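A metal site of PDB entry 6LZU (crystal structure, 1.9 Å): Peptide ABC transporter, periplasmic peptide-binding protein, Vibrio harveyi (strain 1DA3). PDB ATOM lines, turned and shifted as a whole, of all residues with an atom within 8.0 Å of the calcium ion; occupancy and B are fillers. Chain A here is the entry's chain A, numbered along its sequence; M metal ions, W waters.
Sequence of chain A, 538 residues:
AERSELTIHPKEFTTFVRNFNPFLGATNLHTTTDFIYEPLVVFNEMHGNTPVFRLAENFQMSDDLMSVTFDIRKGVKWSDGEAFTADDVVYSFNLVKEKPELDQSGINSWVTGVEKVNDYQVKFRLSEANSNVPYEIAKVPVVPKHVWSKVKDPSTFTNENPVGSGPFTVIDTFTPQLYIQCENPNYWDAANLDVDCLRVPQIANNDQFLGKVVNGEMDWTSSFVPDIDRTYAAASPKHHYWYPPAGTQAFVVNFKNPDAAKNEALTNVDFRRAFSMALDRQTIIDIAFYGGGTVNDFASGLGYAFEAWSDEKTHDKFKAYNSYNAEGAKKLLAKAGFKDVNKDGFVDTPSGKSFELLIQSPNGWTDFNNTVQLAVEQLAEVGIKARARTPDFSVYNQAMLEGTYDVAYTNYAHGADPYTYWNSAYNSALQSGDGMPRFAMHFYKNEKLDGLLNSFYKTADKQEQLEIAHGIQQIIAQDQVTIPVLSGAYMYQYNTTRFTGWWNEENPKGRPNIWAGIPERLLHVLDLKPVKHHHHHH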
ATOM      1  N   LYS A 339     -26.128  10.162 -31.141  1.00  0.00           N
ATOM      2  CA  LYS A 339     -26.899   9.312 -30.242  1.00  0.00           C
ATOM      3  C   LYS A 339     -26.106   8.978 -28.972  1.00  0.00           C
ATOM      4  O   LYS A 339     -24.937   8.650 -29.063  1.00  0.00           O
ATOM      5  CB  LYS A 339     -27.288   8.024 -30.979  1.00  0.00           C
ATOM      6  CG  LYS A 339     -28.118   7.034 -30.177  1.00  0.00           C
ATOM      7  CD  LYS A 339     -28.426   5.805 -31.035  1.00  0.00           C
ATOM      8  CE  LYS A 339     -28.971   4.660 -30.200  1.00  0.00           C
ATOM      9  NZ  LYS A 339     -29.148   3.441 -31.050  1.00  0.00           N
ATOM     10  N   ASP A 340     -26.731   9.079 -27.807  1.00  0.00           N
ATOM     11  CA  ASP A 340     -26.084   8.610 -26.586  1.00  0.00           C
ATOM     12  C   ASP A 340     -26.083   7.073 -26.553  1.00  0.00           C
ATOM     13  O   ASP A 340     -27.134   6.453 -26.436  1.00  0.00           O
ATOM     14  CB  ASP A 340     -26.787   9.153 -25.343  1.00  0.00           C
ATOM     15  CG  ASP A 340     -26.236   8.556 -24.040  1.00  0.00           C
ATOM     16  OD1 ASP A 340     -25.052   8.145 -24.026  1.00  0.00           O
ATOM     17  OD2 ASP A 340     -26.972   8.507 -23.035  1.00  0.00           O
ATOM     18  N   VAL A 341     -24.903   6.458 -26.626  1.00  0.00           N
ATOM     19  CA  VAL A 341     -24.837   5.004 -26.656  1.00  0.00           C
ATOM     20  C   VAL A 341     -24.145   4.391 -25.443  1.00  0.00           C
ATOM     21  O   VAL A 341     -23.838   3.187 -25.448  1.00  0.00           O
ATOM     22  CB  VAL A 341     -24.135   4.505 -27.959  1.00  0.00           C
ATOM     23  CG1 VAL A 341     -25.016   4.801 -29.152  1.00  0.00           C
ATOM     24  CG2 VAL A 341     -22.762   5.162 -28.143  1.00  0.00           C
ATOM     25  N   ASN A 342     -23.896   5.191 -24.396  1.00  0.00           N
ATOM     26  CA  ASN A 342     -23.342   4.629 -23.154  1.00  0.00           C
ATOM     27  C   ASN A 342     -24.047   5.128 -21.904  1.00  0.00           C
ATOM     28  O   ASN A 342     -23.440   5.220 -20.838  1.00  0.00           O
ATOM     29  CB  ASN A 342     -21.833   4.891 -23.062  1.00  0.00           C
ATOM     30  CG  ASN A 342     -21.485   6.371 -22.896  1.00  0.00           C
ATOM     31  OD1 ASN A 342     -22.310   7.239 -23.145  1.00  0.00           O
ATOM     32  ND2 ASN A 342     -20.253   6.640 -22.466  1.00  0.00           N
ATOM     33  N   LYS A 343     -25.337   5.433 -22.055  1.00  0.00           N
ATOM     34  CA  LYS A 343     -26.253   5.610 -20.930  1.00  0.00           C
ATOM     35  C   LYS A 343     -25.864   6.685 -19.918  1.00  0.00           C
ATOM     36  O   LYS A 343     -26.182   6.566 -18.731  1.00  0.00           O
ATOM     37  CB  LYS A 343     -26.430   4.274 -20.191  1.00  0.00           C
ATOM     38  CG  LYS A 343     -26.840   3.133 -21.084  1.00  0.00           C
ATOM     39  CD  LYS A 343     -27.025   1.846 -20.294  1.00  0.00           C
ATOM     40  CE  LYS A 343     -27.219   0.666 -21.220  1.00  0.00           C
ATOM     41  NZ  LYS A 343     -26.071   0.493 -22.160  1.00  0.00           N
ATOM     42  N   ASP A 344     -25.171   7.739 -20.364  1.00  0.00           N
ATOM     43  CA  ASP A 344     -24.757   8.784 -19.447  1.00  0.00           C
ATOM     44  C   ASP A 344     -25.524  10.086 -19.687  1.00  0.00           C
ATOM     45  O   ASP A 344     -25.334  11.087 -18.974  1.00  0.00           O
ATOM     46  CB  ASP A 344     -23.244   8.998 -19.535  1.00  0.00           C
ATOM     47  CG  ASP A 344     -22.804   9.721 -20.801  1.00  0.00           C
ATOM     48  OD1 ASP A 344     -23.583   9.806 -21.797  1.00  0.00           O
ATOM     49  OD2 ASP A 344     -21.653  10.206 -20.808  1.00  0.00           O
ATOM     50  N   GLY A 345     -26.404  10.075 -20.680  1.00  0.00           N
ATOM     51  CA  GLY A 345     -27.248  11.217 -20.973  1.00  0.00           C
ATOM     52  C   GLY A 345     -26.619  12.246 -21.882  1.00  0.00           C
ATOM     53  O   GLY A 345     -27.246  13.252 -22.214  1.00  0.00           O
ATOM     54  N   PHE A 346     -25.370  12.014 -22.285  1.00  0.00           N
ATOM     55  CA  PHE A 346     -24.731  12.950 -23.206  1.00  0.00           C
ATOM     56  C   PHE A 346     -24.527  12.292 -24.568  1.00  0.00           C
ATOM     57  O   PHE A 346     -24.128  11.128 -24.663  1.00  0.00           O
ATOM     58  CB  PHE A 346     -23.385  13.457 -22.630  1.00  0.00           C
ATOM     59  CG  PHE A 346     -23.558  14.339 -21.425  1.00  0.00           C
ATOM     60  CD1 PHE A 346     -23.996  15.655 -21.566  1.00  0.00           C
ATOM     61  CD2 PHE A 346     -23.309  13.856 -20.151  1.00  0.00           C
ATOM     62  CE1 PHE A 346     -24.157  16.489 -20.447  1.00  0.00           C
ATOM     63  CE2 PHE A 346     -23.482  14.674 -19.024  1.00  0.00           C
ATOM     64  CZ  PHE A 346     -23.908  15.985 -19.171  1.00  0.00           C
ATOM     65  N   VAL A 347     -24.843  13.034 -25.632  1.00  0.00           N
ATOM     66  CA  VAL A 347     -24.756  12.434 -26.963  1.00  0.00           C
ATOM     67  C   VAL A 347     -23.321  12.071 -27.317  1.00  0.00           C
ATOM     68  O   VAL A 347     -22.369  12.700 -26.854  1.00  0.00           O
ATOM     69  CB  VAL A 347     -25.311  13.359 -28.040  1.00  0.00           C
ATOM     70  CG1 VAL A 347     -26.746  13.700 -27.705  1.00  0.00           C
ATOM     71  CG2 VAL A 347     -24.456  14.612 -28.156  1.00  0.00           C
ATOM     72  N   ASP A 348     -23.178  11.038 -28.135  1.00  0.00           N
ATOM     73  CA  ASP A 348     -21.883  10.643 -28.632  1.00  0.00           C
ATOM     74  C   ASP A 348     -21.832  10.877 -30.139  1.00  0.00           C
ATOM     75  O   ASP A 348     -22.881  11.078 -30.785  1.00  0.00           O
ATOM     76  CB  ASP A 348     -21.610   9.176 -28.253  1.00  0.00           C
ATOM     77  CG  ASP A 348     -21.792   8.932 -26.754  1.00  0.00           C
ATOM     78  OD1 ASP A 348     -21.031   9.561 -26.000  1.00  0.00           O
ATOM     79  OD2 ASP A 348     -22.680   8.144 -26.330  1.00  0.00           O
ATOM     80  N   THR A 349     -20.633  10.877 -30.709  1.00  0.00           N
ATOM     81  CA  THR A 349     -20.470  11.090 -32.152  1.00  0.00           C
ATOM     82  C   THR A 349     -21.143   9.980 -32.971  1.00  0.00           C
ATOM     83  O   THR A 349     -21.417   8.902 -32.449  1.00  0.00           O
ATOM     84  CB  THR A 349     -18.984  11.150 -32.547  1.00  0.00           C
ATOM     85  OG1 THR A 349     -18.413   9.847 -32.465  1.00  0.00           O
ATOM     86  CG2 THR A 349     -18.223  12.143 -31.651  1.00  0.00           C
ATOM     87  N   GLY A 352     -19.647   6.713 -32.583  1.00  0.00           N
ATOM     88  CA  GLY A 352     -19.820   6.067 -31.291  1.00  0.00           C
ATOM     89  C   GLY A 352     -18.936   6.585 -30.166  1.00  0.00           C
ATOM     90  O   GLY A 352     -18.910   5.994 -29.077  1.00  0.00           O
ATOM     91  N   LYS A 353     -18.235   7.691 -30.382  1.00  0.00           N
ATOM     92  CA  LYS A 353     -17.281   8.144 -29.365  1.00  0.00           C
ATOM     93  C   LYS A 353     -17.846   9.207 -28.459  1.00  0.00           C
ATOM     94  O   LYS A 353     -18.505  10.159 -28.901  1.00  0.00           O
ATOM     95  CB  LYS A 353     -16.007   8.686 -30.017  1.00  0.00           C
ATOM     96  CG  LYS A 353     -15.308   7.721 -30.930  1.00  0.00           C
ATOM     97  CD  LYS A 353     -14.060   8.380 -31.510  1.00  0.00           C
ATOM     98  CE  LYS A 353     -13.307   7.438 -32.439  1.00  0.00           C
ATOM     99  NZ  LYS A 353     -13.985   7.356 -33.762  1.00  0.00           N
ATOM    100  N   SER A 354     -17.566   9.061 -27.172  1.00  0.00           N
ATOM    101  CA  SER A 354     -17.913  10.094 -26.212  1.00  0.00           C
ATOM    102  C   SER A 354     -16.916  11.242 -26.275  1.00  0.00           C
ATOM    103  O   SER A 354     -15.774  11.085 -26.709  1.00  0.00           O
ATOM    104  CB  SER A 354     -17.984   9.508 -24.807  1.00  0.00           C
ATOM    105  OG  SER A 354     -19.092   8.628 -24.737  1.00  0.00           O
ATOM    106  N   PHE A 355     -17.364  12.409 -25.840  1.00  0.00           N
ATOM    107  CA  PHE A 355     -16.539  13.603 -25.848  1.00  0.00           C
ATOM    108  C   PHE A 355     -17.093  14.649 -24.910  1.00  0.00           C
ATOM    109  O   PHE A 355     -18.278  14.628 -24.573  1.00  0.00           O
ATOM    110  CB  PHE A 355     -16.422  14.186 -27.260  1.00  0.00           C
ATOM    111  CG  PHE A 355     -17.742  14.664 -27.831  1.00  0.00           C
ATOM    112  CD1 PHE A 355     -18.629  13.784 -28.427  1.00  0.00           C
ATOM    113  CD2 PHE A 355     -18.064  16.012 -27.807  1.00  0.00           C
ATOM    114  CE1 PHE A 355     -19.820  14.239 -28.972  1.00  0.00           C
ATOM    115  CE2 PHE A 355     -19.267  16.473 -28.348  1.00  0.00           C
ATOM    116  CZ  PHE A 355     -20.134  15.590 -28.931  1.00  0.00           C
ATOM    117  N   GLY A 383     -28.197  17.535 -23.912  1.00  0.00           N
ATOM    118  CA  GLY A 383     -27.349  16.360 -23.979  1.00  0.00           C
ATOM    119  C   GLY A 383     -25.992  16.558 -24.614  1.00  0.00           C
ATOM    120  O   GLY A 383     -25.354  15.598 -25.018  1.00  0.00           O
ATOM    121  N   LYS A 385     -22.204  17.490 -23.778  1.00  0.00           N
ATOM    122  CA  LYS A 385     -21.333  17.634 -22.614  1.00  0.00           C
ATOM    123  C   LYS A 385     -20.241  18.663 -22.853  1.00  0.00           C
ATOM    124  O   LYS A 385     -19.524  18.607 -23.867  1.00  0.00           O
ATOM    125  CB  LYS A 385     -20.692  16.287 -22.258  1.00  0.00           C
ATOM    126  CG  LYS A 385     -20.239  16.187 -20.822  1.00  0.00           C
ATOM    127  CD  LYS A 385     -19.659  14.807 -20.545  1.00  0.00           C
ATOM    128  CE  LYS A 385     -19.258  14.620 -19.096  1.00  0.00           C
ATOM    129  NZ  LYS A 385     -18.588  13.291 -18.931  1.00  0.00           N
HETATM  130 CA    CA M   1     -22.958   9.245 -24.036  1.00  0.00          CA
HETATM  131  O   HOH W   1     -21.120  10.496 -23.081  1.00  0.00           O
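The side-chain hydroxyl (OG) of Ser 354 sits at hydrogen-bond distance from the side-chain amide nitrogen (ND2) of Asn 342 (3.2 Å).
The side-chain carboxylate of Asp 340 sits at hydrogen-bond distance from the backbone NH of Gly 345 (2.9 Å).
The backbone NH of Lys 343 lies close to the side-chain carboxylate of Asp 340 (3.4 Å).
OD1 of Asp 348 sits close to OG of Ser 354 (2.5 Å).
The side-chain carboxylate (OD2) of Asp 348 sits close to the backbone NH (N) of Val 341 (2.8 Å).
O of Lys 339 lies within hydrogen-bond range of N of Asp 348.
Merely in contact with the calcium ion: Ser 354.
The nearest printed residue that does not touch the calcium ion is Val 341 (4.3 Å).
The calcium ion is bound by OD1 of Asn 342 (2.3 Å), O of Phe 346 (2.3 Å), OD1 of Asp 340 (2.4 Å), OD1 of Asp 344 (2.4 Å), water W1 (2.4 Å), OD2 of Asp 348 (2.6 Å) and OD1 of Asp 348 (2.8 Å).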
